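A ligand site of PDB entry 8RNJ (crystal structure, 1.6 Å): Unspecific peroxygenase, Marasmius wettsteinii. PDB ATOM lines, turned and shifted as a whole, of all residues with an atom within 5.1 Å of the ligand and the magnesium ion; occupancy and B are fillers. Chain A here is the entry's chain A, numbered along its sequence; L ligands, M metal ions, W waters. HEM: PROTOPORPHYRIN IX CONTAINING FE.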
ATOM      1  N   PRO A  20     -34.320  28.663 -13.039  1.00  0.00           N
ATOM      2  CA  PRO A  20     -34.113  29.184 -11.687  1.00  0.00           C
ATOM      3  C   PRO A  20     -32.690  29.028 -11.135  1.00  0.00           C
ATOM      4  O   PRO A  20     -32.414  29.415 -10.001  1.00  0.00           O
ATOM      5  CB  PRO A  20     -35.103  28.314 -10.893  1.00  0.00           C
ATOM      6  CG  PRO A  20     -35.011  26.968 -11.570  1.00  0.00           C
ATOM      7  CD  PRO A  20     -34.915  27.312 -13.054  1.00  0.00           C
ATOM      8  N   CYS A  21     -31.792  28.440 -11.950  1.00  0.00           N
ATOM      9  CA  CYS A  21     -30.419  28.156 -11.569  1.00  0.00           C
ATOM     10  C   CYS A  21     -29.470  29.191 -12.147  1.00  0.00           C
ATOM     11  O   CYS A  21     -29.236  29.208 -13.355  1.00  0.00           O
ATOM     12  CB  CYS A  21     -29.989  26.782 -12.069  1.00  0.00           C
ATOM     13  SG  CYS A  21     -28.252  26.423 -11.706  1.00  0.00           S
ATOM     14  N   PRO A  22     -28.800  30.014 -11.306  1.00  0.00           N
ATOM     15  CA  PRO A  22     -27.789  30.946 -11.793  1.00  0.00           C
ATOM     16  C   PRO A  22     -26.554  30.271 -12.364  1.00  0.00           C
ATOM     17  O   PRO A  22     -25.886  30.837 -13.235  1.00  0.00           O
ATOM     18  CB  PRO A  22     -27.433  31.795 -10.554  1.00  0.00           C
ATOM     19  CG  PRO A  22     -27.817  30.901  -9.381  1.00  0.00           C
ATOM     20  CD  PRO A  22     -29.006  30.102  -9.858  1.00  0.00           C
ATOM     21  N   GLY A  23     -26.234  29.062 -11.890  1.00  0.00           N
ATOM     22  CA  GLY A  23     -25.078  28.328 -12.389  1.00  0.00           C
ATOM     23  C   GLY A  23     -25.227  27.985 -13.874  1.00  0.00           C
ATOM     24  O   GLY A  23     -24.340  28.293 -14.680  1.00  0.00           O
ATOM     25  N   LEU A  24     -26.359  27.371 -14.232  1.00  0.00           N
ATOM     26  CA  LEU A  24     -26.577  26.967 -15.618  1.00  0.00           C
ATOM     27  C   LEU A  24     -26.899  28.196 -16.478  1.00  0.00           C
ATOM     28  O   LEU A  24     -26.447  28.270 -17.623  1.00  0.00           O
ATOM     29  CB  LEU A  24     -27.673  25.913 -15.683  1.00  0.00           C
ATOM     30  CG  LEU A  24     -27.381  24.613 -14.931  1.00  0.00           C
ATOM     31  CD1 LEU A  24     -28.572  23.669 -15.089  1.00  0.00           C
ATOM     32  CD2 LEU A  24     -26.092  23.946 -15.409  1.00  0.00           C
ATOM     33  N   ILE A  45     -23.946  19.424 -19.930  1.00  0.00           N
ATOM     34  CA  ILE A  45     -23.782  20.058 -18.622  1.00  0.00           C
ATOM     35  C   ILE A  45     -22.437  19.688 -18.008  1.00  0.00           C
ATOM     36  O   ILE A  45     -21.736  20.537 -17.467  1.00  0.00           O
ATOM     37  CB  ILE A  45     -24.956  19.689 -17.701  1.00  0.00           C
ATOM     38  CG1 ILE A  45     -26.246  20.339 -18.197  1.00  0.00           C
ATOM     39  CG2 ILE A  45     -24.642  20.069 -16.263  1.00  0.00           C
ATOM     40  CD1 ILE A  45     -27.488  19.849 -17.478  1.00  0.00           C
ATOM     41  N   TYR A  53     -16.284  26.281 -14.793  1.00  0.00           N
ATOM     42  CA  TYR A  53     -16.152  26.406 -13.346  1.00  0.00           C
ATOM     43  C   TYR A  53     -15.173  25.423 -12.712  1.00  0.00           C
ATOM     44  O   TYR A  53     -14.919  25.529 -11.518  1.00  0.00           O
ATOM     45  CB  TYR A  53     -17.506  26.175 -12.657  1.00  0.00           C
ATOM     46  CG  TYR A  53     -18.664  27.054 -13.068  1.00  0.00           C
ATOM     47  CD1 TYR A  53     -18.529  28.420 -13.246  1.00  0.00           C
ATOM     48  CD2 TYR A  53     -19.945  26.535 -13.164  1.00  0.00           C
ATOM     49  CE1 TYR A  53     -19.611  29.226 -13.539  1.00  0.00           C
ATOM     50  CE2 TYR A  53     -21.050  27.320 -13.457  1.00  0.00           C
ATOM     51  CZ  TYR A  53     -20.877  28.682 -13.665  1.00  0.00           C
ATOM     52  OH  TYR A  53     -21.967  29.447 -13.958  1.00  0.00           O
ATOM     53  N   VAL A  55     -16.061  22.399 -12.202  1.00  0.00           N
ATOM     54  CA  VAL A  55     -16.912  21.486 -11.457  1.00  0.00           C
ATOM     55  C   VAL A  55     -16.881  20.126 -12.150  1.00  0.00           C
ATOM     56  O   VAL A  55     -16.985  20.046 -13.369  1.00  0.00           O
ATOM     57  CB  VAL A  55     -18.342  22.021 -11.290  1.00  0.00           C
ATOM     58  CG1 VAL A  55     -19.292  20.983 -10.666  1.00  0.00           C
ATOM     59  CG2 VAL A  55     -18.362  23.305 -10.454  1.00  0.00           C
ATOM     60  N   ILE A  59     -20.825  15.384  -9.325  1.00  0.00           N
ATOM     61  CA  ILE A  59     -21.986  16.137  -8.869  1.00  0.00           C
ATOM     62  C   ILE A  59     -22.903  16.455 -10.057  1.00  0.00           C
ATOM     63  O   ILE A  59     -24.120  16.489  -9.907  1.00  0.00           O
ATOM     64  CB  ILE A  59     -21.619  17.390  -8.049  1.00  0.00           C
ATOM     65  CG1 ILE A  59     -22.864  18.178  -7.611  1.00  0.00           C
ATOM     66  CG2 ILE A  59     -20.676  18.293  -8.816  1.00  0.00           C
ATOM     67  CD1 ILE A  59     -23.875  17.395  -6.788  1.00  0.00           C
ATOM     68  N   LEU A  60     -22.329  16.746 -11.228  1.00  0.00           N
ATOM     69  CA  LEU A  60     -23.147  17.158 -12.350  1.00  0.00           C
ATOM     70  C   LEU A  60     -23.951  15.997 -12.947  1.00  0.00           C
ATOM     71  O   LEU A  60     -25.033  16.243 -13.452  1.00  0.00           O
ATOM     72  CB  LEU A  60     -22.269  17.827 -13.410  1.00  0.00           C
ATOM     73  CG  LEU A  60     -21.619  19.130 -12.926  1.00  0.00           C
ATOM     74  CD1 LEU A  60     -20.687  19.696 -13.999  1.00  0.00           C
ATOM     75  CD2 LEU A  60     -22.663  20.156 -12.528  1.00  0.00           C
ATOM     76  N   ALA A  63     -26.937  15.483 -10.240  1.00  0.00           N
ATOM     77  CA  ALA A  63     -27.912  16.556 -10.315  1.00  0.00           C
ATOM     78  C   ALA A  63     -28.507  16.649 -11.726  1.00  0.00           C
ATOM     79  O   ALA A  63     -29.715  16.854 -11.857  1.00  0.00           O
ATOM     80  CB  ALA A  63     -27.242  17.845  -9.908  1.00  0.00           C
ATOM     81  N   GLY A  64     -27.676  16.452 -12.748  1.00  0.00           N
ATOM     82  CA  GLY A  64     -28.137  16.532 -14.122  1.00  0.00           C
ATOM     83  C   GLY A  64     -29.256  15.542 -14.441  1.00  0.00           C
ATOM     84  O   GLY A  64     -30.235  15.918 -15.069  1.00  0.00           O
ATOM     85  N   GLY A  67     -32.386  16.604 -12.914  1.00  0.00           N
ATOM     86  CA  GLY A  67     -32.902  17.712 -13.706  1.00  0.00           C
ATOM     87  C   GLY A  67     -33.590  17.270 -15.001  1.00  0.00           C
ATOM     88  O   GLY A  67     -34.573  17.882 -15.415  1.00  0.00           O
ATOM     89  N   LEU A  82     -36.518  23.496 -15.571  1.00  0.00           N
ATOM     90  CA  LEU A  82     -36.012  23.221 -14.235  1.00  0.00           C
ATOM     91  C   LEU A  82     -36.783  23.956 -13.141  1.00  0.00           C
ATOM     92  O   LEU A  82     -36.574  23.679 -11.948  1.00  0.00           O
ATOM     93  CB  LEU A  82     -34.532  23.605 -14.180  1.00  0.00           C
ATOM     94  CG  LEU A  82     -33.562  22.713 -14.951  1.00  0.00           C
ATOM     95  CD1 LEU A  82     -32.170  23.348 -14.959  1.00  0.00           C
ATOM     96  CD2 LEU A  82     -33.472  21.324 -14.323  1.00  0.00           C
ATOM     97  N   ILE A  88     -36.220  19.522  -8.346  1.00  0.00           N
ATOM     98  CA  ILE A  88     -35.134  20.196  -7.647  1.00  0.00           C
ATOM     99  C   ILE A  88     -35.633  21.519  -7.063  1.00  0.00           C
ATOM    100  O   ILE A  88     -35.355  21.817  -5.897  1.00  0.00           O
ATOM    101  CB  ILE A  88     -33.922  20.411  -8.578  1.00  0.00           C
ATOM    102  CG1 ILE A  88     -33.320  19.080  -9.058  1.00  0.00           C
ATOM    103  CG2 ILE A  88     -32.861  21.291  -7.917  1.00  0.00           C
ATOM    104  CD1 ILE A  88     -32.272  19.193 -10.130  1.00  0.00           C
ATOM    105  N   GLU A  89     -36.388  22.299  -7.850  1.00  0.00           N
ATOM    106  CA  GLU A  89     -36.849  23.618  -7.441  1.00  0.00           C
ATOM    107  C   GLU A  89     -37.643  23.526  -6.125  1.00  0.00           C
ATOM    108  O   GLU A  89     -38.471  22.633  -5.958  1.00  0.00           O
ATOM    109  CB  GLU A  89     -37.668  24.290  -8.545  1.00  0.00           C
ATOM    110  CG  GLU A  89     -37.875  25.777  -8.346  1.00  0.00           C
ATOM    111  CD  GLU A  89     -38.894  26.138  -7.278  1.00  0.00           C
ATOM    112  OE1 GLU A  89     -39.955  25.509  -7.262  1.00  0.00           O
ATOM    113  OE2 GLU A  89     -38.648  27.053  -6.456  1.00  0.00           O
ATOM    114  N   HIS A  90     -37.316  24.423  -5.191  1.00  0.00           N
ATOM    115  CA  HIS A  90     -37.776  24.357  -3.807  1.00  0.00           C
ATOM    116  C   HIS A  90     -38.124  25.755  -3.299  1.00  0.00           C
ATOM    117  O   HIS A  90     -37.611  26.767  -3.792  1.00  0.00           O
ATOM    118  CB  HIS A  90     -36.684  23.736  -2.919  1.00  0.00           C
ATOM    119  CG  HIS A  90     -35.374  24.432  -3.067  1.00  0.00           C
ATOM    120  ND1 HIS A  90     -35.135  25.669  -2.518  1.00  0.00           N
ATOM    121  CD2 HIS A  90     -34.257  24.092  -3.730  1.00  0.00           C
ATOM    122  CE1 HIS A  90     -33.929  26.072  -2.895  1.00  0.00           C
ATOM    123  NE2 HIS A  90     -33.362  25.126  -3.580  1.00  0.00           N
ATOM    124  N   ASP A  91     -38.911  25.794  -2.229  1.00  0.00           N
ATOM    125  CA  ASP A  91     -39.139  27.012  -1.461  1.00  0.00           C
ATOM    126  C   ASP A  91     -37.884  27.476  -0.719  1.00  0.00           C
ATOM    127  O   ASP A  91     -36.911  26.712  -0.555  1.00  0.00           O
ATOM    128  CB  ASP A  91     -40.262  26.758  -0.452  1.00  0.00           C
ATOM    129  CG  ASP A  91     -41.582  26.336  -1.097  1.00  0.00           C
ATOM    130  OD1 ASP A  91     -41.851  26.789  -2.218  1.00  0.00           O
ATOM    131  OD2 ASP A  91     -42.347  25.515  -0.479  1.00  0.00           O
ATOM    132  N   SER A  93     -35.664  29.741  -1.615  1.00  0.00           N
ATOM    133  CA  SER A  93     -34.546  30.066  -2.495  1.00  0.00           C
ATOM    134  C   SER A  93     -33.860  31.353  -2.049  1.00  0.00           C
ATOM    135  O   SER A  93     -34.461  32.169  -1.350  1.00  0.00           O
ATOM    136  CB  SER A  93     -35.000  30.179  -3.923  1.00  0.00           C
ATOM    137  OG  SER A  93     -35.423  28.917  -4.424  1.00  0.00           O
ATOM    138  N   LEU A  94     -32.623  31.523  -2.521  1.00  0.00           N
ATOM    139  CA  LEU A  94     -31.776  32.674  -2.184  1.00  0.00           C
ATOM    140  C   LEU A  94     -32.184  33.930  -2.971  1.00  0.00           C
ATOM    141  O   LEU A  94     -31.921  35.035  -2.500  1.00  0.00           O
ATOM    142  CB  LEU A  94     -30.326  32.325  -2.500  1.00  0.00           C
ATOM    143  CG  LEU A  94     -29.734  31.192  -1.663  1.00  0.00           C
ATOM    144  CD1 LEU A  94     -28.403  30.743  -2.227  1.00  0.00           C
ATOM    145  CD2 LEU A  94     -29.564  31.601  -0.205  1.00  0.00           C
ATOM    146  N   SER A  95     -32.731  33.749  -4.168  1.00  0.00           N
ATOM    147  CA  SER A  95     -32.942  34.869  -5.086  1.00  0.00           C
ATOM    148  C   SER A  95     -34.264  34.778  -5.861  1.00  0.00           C
ATOM    149  O   SER A  95     -34.519  35.601  -6.742  1.00  0.00           O
ATOM    150  CB  SER A  95     -31.765  34.973  -6.033  1.00  0.00           C
ATOM    151  OG  SER A  95     -31.712  33.891  -6.953  1.00  0.00           O
ATOM    152  N   ARG A  96     -35.096  33.755  -5.571  1.00  0.00           N
ATOM    153  CA  ARG A  96     -36.400  33.562  -6.192  1.00  0.00           C
ATOM    154  C   ARG A  96     -37.471  33.464  -5.111  1.00  0.00           C
ATOM    155  O   ARG A  96     -37.154  33.187  -3.960  1.00  0.00           O
ATOM    156  CB  ARG A  96     -36.422  32.259  -7.013  1.00  0.00           C
ATOM    157  CG  ARG A  96     -35.958  32.371  -8.457  1.00  0.00           C
ATOM    158  CD  ARG A  96     -34.510  32.757  -8.648  1.00  0.00           C
ATOM    159  NE  ARG A  96     -34.119  32.673 -10.046  1.00  0.00           N
ATOM    160  CZ  ARG A  96     -32.952  33.068 -10.544  1.00  0.00           C
ATOM    161  NH1 ARG A  96     -32.019  33.585  -9.773  1.00  0.00           N
ATOM    162  NH2 ARG A  96     -32.730  32.981 -11.853  1.00  0.00           N
ATOM    163  N   GLU A  97     -38.730  33.728  -5.492  1.00  0.00           N
ATOM    164  CA  GLU A  97     -39.882  33.610  -4.608  1.00  0.00           C
ATOM    165  C   GLU A  97     -40.392  32.164  -4.616  1.00  0.00           C
ATOM    166  O   GLU A  97     -40.137  31.426  -5.570  1.00  0.00           O
ATOM    167  CB  GLU A  97     -41.017  34.529  -5.049  1.00  0.00           C
ATOM    168  CG  GLU A  97     -40.619  35.998  -5.087  1.00  0.00           C
ATOM    169  CD  GLU A  97     -41.692  36.938  -5.603  1.00  0.00           C
ATOM    170  OE1 GLU A  97     -42.269  36.655  -6.674  1.00  0.00           O
ATOM    171  OE2 GLU A  97     -41.928  37.970  -4.928  1.00  0.00           O
ATOM    172  N   ASN A 104     -41.216  31.672  -9.057  1.00  0.00           N
ATOM    173  CA  ASN A 104     -40.151  30.768  -8.634  1.00  0.00           C
ATOM    174  C   ASN A 104     -39.046  30.631  -9.675  1.00  0.00           C
ATOM    175  O   ASN A 104     -38.145  29.796  -9.487  1.00  0.00           O
ATOM    176  CB  ASN A 104     -40.689  29.376  -8.269  1.00  0.00           C
ATOM    177  CG  ASN A 104     -41.095  28.572  -9.486  1.00  0.00           C
ATOM    178  OD1 ASN A 104     -41.387  29.133 -10.530  1.00  0.00           O
ATOM    179  ND2 ASN A 104     -41.143  27.252  -9.362  1.00  0.00           N
ATOM    180  N   GLU A 161     -26.506  24.399  -2.905  1.00  0.00           N
ATOM    181  CA  GLU A 161     -26.532  25.617  -3.707  1.00  0.00           C
ATOM    182  C   GLU A 161     -25.686  26.704  -3.047  1.00  0.00           C
ATOM    183  O   GLU A 161     -24.936  27.406  -3.728  1.00  0.00           O
ATOM    184  CB  GLU A 161     -27.993  25.972  -3.965  1.00  0.00           C
ATOM    185  CG  GLU A 161     -28.630  24.953  -4.892  1.00  0.00           C
ATOM    186  CD  GLU A 161     -30.138  24.821  -4.935  1.00  0.00           C
ATOM    187  OE1 GLU A 161     -30.799  25.488  -4.147  1.00  0.00           O
ATOM    188  OE2 GLU A 161     -30.633  24.057  -5.795  1.00  0.00           O
ATOM    189  N   PHE A 164     -22.161  25.871  -3.633  1.00  0.00           N
ATOM    190  CA  PHE A 164     -21.794  26.193  -4.995  1.00  0.00           C
ATOM    191  C   PHE A 164     -21.378  27.661  -5.116  1.00  0.00           C
ATOM    192  O   PHE A 164     -20.322  27.928  -5.717  1.00  0.00           O
ATOM    193  CB  PHE A 164     -22.931  25.889  -5.978  1.00  0.00           C
ATOM    194  CG  PHE A 164     -22.842  24.555  -6.661  1.00  0.00           C
ATOM    195  CD1 PHE A 164     -21.634  24.086  -7.148  1.00  0.00           C
ATOM    196  CD2 PHE A 164     -23.983  23.804  -6.895  1.00  0.00           C
ATOM    197  CE1 PHE A 164     -21.546  22.882  -7.823  1.00  0.00           C
ATOM    198  CE2 PHE A 164     -23.900  22.592  -7.568  1.00  0.00           C
ATOM    199  CZ  PHE A 164     -22.680  22.133  -8.021  1.00  0.00           C
ATOM    200  N   TYR A 165     -22.151  28.611  -4.578  1.00  0.00           N
ATOM    201  CA  TYR A 165     -21.779  30.010  -4.778  1.00  0.00           C
ATOM    202  C   TYR A 165     -20.485  30.302  -4.018  1.00  0.00           C
ATOM    203  O   TYR A 165     -19.670  31.078  -4.514  1.00  0.00           O
ATOM    204  CB  TYR A 165     -22.920  31.010  -4.526  1.00  0.00           C
ATOM    205  CG  TYR A 165     -23.261  31.373  -3.100  1.00  0.00           C
ATOM    206  CD1 TYR A 165     -22.420  32.146  -2.306  1.00  0.00           C
ATOM    207  CD2 TYR A 165     -24.493  30.998  -2.574  1.00  0.00           C
ATOM    208  CE1 TYR A 165     -22.778  32.486  -1.011  1.00  0.00           C
ATOM    209  CE2 TYR A 165     -24.871  31.358  -1.293  1.00  0.00           C
ATOM    210  CZ  TYR A 165     -24.013  32.108  -0.508  1.00  0.00           C
ATOM    211  OH  TYR A 165     -24.393  32.412   0.771  1.00  0.00           O
ATOM    212  N   VAL A 168     -17.532  28.076  -6.432  1.00  0.00           N
ATOM    213  CA  VAL A 168     -17.340  28.401  -7.832  1.00  0.00           C
ATOM    214  C   VAL A 168     -16.916  29.869  -7.995  1.00  0.00           C
ATOM    215  O   VAL A 168     -16.143  30.157  -8.909  1.00  0.00           O
ATOM    216  CB  VAL A 168     -18.594  28.075  -8.657  1.00  0.00           C
ATOM    217  CG1 VAL A 168     -18.512  28.592 -10.062  1.00  0.00           C
ATOM    218  CG2 VAL A 168     -18.885  26.570  -8.670  1.00  0.00           C
ATOM    219  N   PHE A 187     -22.640  37.236 -10.083  1.00  0.00           N
ATOM    220  CA  PHE A 187     -23.157  35.912 -10.438  1.00  0.00           C
ATOM    221  C   PHE A 187     -24.683  35.883 -10.346  1.00  0.00           C
ATOM    222  O   PHE A 187     -25.348  35.496 -11.297  1.00  0.00           O
ATOM    223  CB  PHE A 187     -22.446  34.883  -9.542  1.00  0.00           C
ATOM    224  CG  PHE A 187     -22.909  33.455  -9.697  1.00  0.00           C
ATOM    225  CD1 PHE A 187     -22.603  32.727 -10.837  1.00  0.00           C
ATOM    226  CD2 PHE A 187     -23.618  32.855  -8.683  1.00  0.00           C
ATOM    227  CE1 PHE A 187     -23.012  31.414 -10.959  1.00  0.00           C
ATOM    228  CE2 PHE A 187     -24.049  31.542  -8.812  1.00  0.00           C
ATOM    229  CZ  PHE A 187     -23.722  30.814  -9.945  1.00  0.00           C
ATOM    230  N   PHE A 188     -25.258  36.288  -9.213  1.00  0.00           N
ATOM    231  CA  PHE A 188     -26.700  36.272  -9.031  1.00  0.00           C
ATOM    232  C   PHE A 188     -27.416  37.366  -9.829  1.00  0.00           C
ATOM    233  O   PHE A 188     -28.399  37.094 -10.504  1.00  0.00           O
ATOM    234  CB  PHE A 188     -27.071  36.403  -7.554  1.00  0.00           C
ATOM    235  CG  PHE A 188     -27.003  35.126  -6.750  1.00  0.00           C
ATOM    236  CD1 PHE A 188     -28.087  34.271  -6.694  1.00  0.00           C
ATOM    237  CD2 PHE A 188     -25.855  34.820  -6.024  1.00  0.00           C
ATOM    238  CE1 PHE A 188     -28.008  33.095  -5.956  1.00  0.00           C
ATOM    239  CE2 PHE A 188     -25.788  33.651  -5.282  1.00  0.00           C
ATOM    240  CZ  PHE A 188     -26.875  32.809  -5.231  1.00  0.00           C
HETATM  241  CHA HEM L   1     -30.437  26.582  -7.960  1.00  0.00           C
HETATM  242  CHB HEM L   1     -30.543  22.859 -11.002  1.00  0.00           C
HETATM  243  CHC HEM L   1     -25.753  23.171 -11.500  1.00  0.00           C
HETATM  244  CHD HEM L   1     -25.663  26.959  -8.553  1.00  0.00           C
HETATM  245  C1A HEM L   1     -30.877  25.593  -8.787  1.00  0.00           C
HETATM  246  C2A HEM L   1     -32.227  25.296  -8.986  1.00  0.00           C
HETATM  247  C3A HEM L   1     -32.285  24.272  -9.874  1.00  0.00           C
HETATM  248  C4A HEM L   1     -30.940  23.892 -10.180  1.00  0.00           C
HETATM  249  CMA HEM L   1     -33.524  23.620 -10.420  1.00  0.00           C
HETATM  250  CAA HEM L   1     -33.395  26.030  -8.391  1.00  0.00           C
HETATM  251  CBA HEM L   1     -33.638  25.564  -6.958  1.00  0.00           C
HETATM  252  CGA HEM L   1     -34.285  26.639  -6.134  1.00  0.00           C
HETATM  253  O1A HEM L   1     -35.496  26.573  -5.923  1.00  0.00           O
HETATM  254  O2A HEM L   1     -33.627  27.589  -5.698  1.00  0.00           O
HETATM  255  C1B HEM L   1     -29.233  22.618 -11.370  1.00  0.00           C
HETATM  256  C2B HEM L   1     -28.853  21.532 -12.212  1.00  0.00           C
HETATM  257  C3B HEM L   1     -27.510  21.618 -12.397  1.00  0.00           C
HETATM  258  C4B HEM L   1     -27.066  22.771 -11.560  1.00  0.00           C
HETATM  259  CMB HEM L   1     -29.764  20.534 -12.848  1.00  0.00           C
HETATM  260  CAB HEM L   1     -26.571  20.686 -13.097  1.00  0.00           C
HETATM  261  CBB HEM L   1     -26.385  19.467 -12.731  1.00  0.00           C
HETATM  262  C1C HEM L   1     -25.288  24.245 -10.783  1.00  0.00           C
HETATM  263  C2C HEM L   1     -23.991  24.765 -10.838  1.00  0.00           C
HETATM  264  C3C HEM L   1     -23.943  25.836  -9.982  1.00  0.00           C
HETATM  265  C4C HEM L   1     -25.262  26.018  -9.440  1.00  0.00           C
HETATM  266  CMC HEM L   1     -22.819  24.208 -11.628  1.00  0.00           C
HETATM  267  CAC HEM L   1     -22.704  26.605  -9.800  1.00  0.00           C
HETATM  268  CBC HEM L   1     -22.598  27.766  -9.257  1.00  0.00           C
HETATM  269  C1D HEM L   1     -26.996  27.132  -8.112  1.00  0.00           C
HETATM  270  C2D HEM L   1     -27.381  28.120  -7.092  1.00  0.00           C
HETATM  271  C3D HEM L   1     -28.715  28.025  -6.935  1.00  0.00           C
HETATM  272  C4D HEM L   1     -29.125  26.933  -7.849  1.00  0.00           C
HETATM  273  CMD HEM L   1     -26.443  29.081  -6.378  1.00  0.00           C
HETATM  274  CAD HEM L   1     -29.582  28.807  -5.967  1.00  0.00           C
HETATM  275  CBD HEM L   1     -30.491  29.830  -6.604  1.00  0.00           C
HETATM  276  CGD HEM L   1     -31.383  30.413  -5.518  1.00  0.00           C
HETATM  277  O1D HEM L   1     -31.995  31.485  -5.727  1.00  0.00           O
HETATM  278  O2D HEM L   1     -31.497  29.883  -4.375  1.00  0.00           O
HETATM  279  NA  HEM L   1     -30.080  24.724  -9.535  1.00  0.00           N
HETATM  280  NB  HEM L   1     -28.147  23.285 -10.991  1.00  0.00           N
HETATM  281  NC  HEM L   1     -26.056  25.037  -9.976  1.00  0.00           N
HETATM  282  ND  HEM L   1     -28.070  26.437  -8.544  1.00  0.00           N
HETATM  283 FE   HEM L   1     -28.129  25.010  -9.822  1.00  0.00          FE
HETATM  284 MG    MG M   1     -37.096  27.959  -5.528  1.00  0.00          MG
HETATM  285  O   HOH W   1     -27.890  23.580  -8.061  1.00  0.00           O
HETATM  286  O   HOH W   2     -38.331  29.507  -4.847  1.00  0.00           O
HETATM  287  O   HOH W   3     -31.137  27.721  -2.723  1.00  0.00           O
HETATM  288  O   HOH W   4     -36.579  28.946  -7.302  1.00  0.00           O
HETATM  289  O   HOH W   5     -34.059  29.712  -7.773  1.00  0.00           O
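Merely in contact with the ligand: Gly 64, Phe 187, Glu 161, Ala 63, Leu 82, Ile 88, Leu 24, Leu 60, Pro 22, Phe 164, Gly 23, Pro 20, Ile 45, Arg 96, Phe 188 and Val 168. 22 residues have an atom within 4 Å of the ligand: Pro 20, Cys 21, Pro 22, Gly 23, Leu 24, Ile 45, Leu 60, Ala 63, Gly 64, Leu 82, Ile 88, Glu 89, His 90, Ser 93, Leu 94, Ser 95, Arg 96, Glu 161, Phe 164, Val 168, Phe 187 and Phe 188. The nearest printed residue that does not touch the ligand is Tyr 53 (4.004 Å).
Of the 30 residues printed, 3 come within 4 Å of the magnesium ion. The nearest printed residue that does not touch the magnesium ion is Asp 91 (4.3 Å).
Water W3 bridges OE1 of Glu 161 and O2D of the ligand. Water W5 bridges O of Pro 20 (2.8 Å) and O2A of the ligand (3.0 Å).
The side-chain sulfur (SG) of Cys 21 sits close to the backbone NH (N) of Gly 23, at 3.3 Å. The side-chain hydroxyl of Ser 95 sits at hydrogen-bond distance from the guanidinium group of Arg 96 (2.9 Å). N of Leu 24 sits close to SG of Cys 21 (3.3 Å). The side-chain hydroxyl (OH) of Tyr 53 sits at hydrogen-bond distance from the backbone carbonyl oxygen (O) of Gly 23, 2.7 Å away. ND2 of Asn 104 lies within hydrogen-bond range of OE1 of Glu 89 (3.0 Å). NE2 of His 90 sits at hydrogen-bond distance from OE1 of Glu 161, 2.6 Å away.
The magnesium ion is bound by the side-chain carboxylate of Glu 89 (2.0 Å), water W2 (2.1 Å), water W4 (2.1 Å), an oxygen (O1A) of the ligand (2.2 Å), the backbone carbonyl oxygen of His 90 (2.2 Å) and the side-chain hydroxyl of Ser 93 (2.2 Å). The magnesium ion has six donor atoms within binding distance.
The side-chain hydroxyl (OG) of Ser 95 sits at hydrogen-bond distance from an oxygen (O1D) of the ligand, at 2.7 Å. N of His 90 lies close to O1A of the ligand (2.9 Å). An iron atom (FE) of the ligand is bound by the side-chain sulfur of Cys 21 (2.4 Å). The backbone NH (N) of Ser 95 is in hydrogen-bond range of an oxygen (O1D) of the ligand. An oxygen (O2D) of the ligand is in hydrogen-bond range of the backbone NH of Leu 94 (2.7 Å). A ring nitrogen (NE2) of His 90 sits close to an oxygen (O2A) of the ligand, 3.3 Å away.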
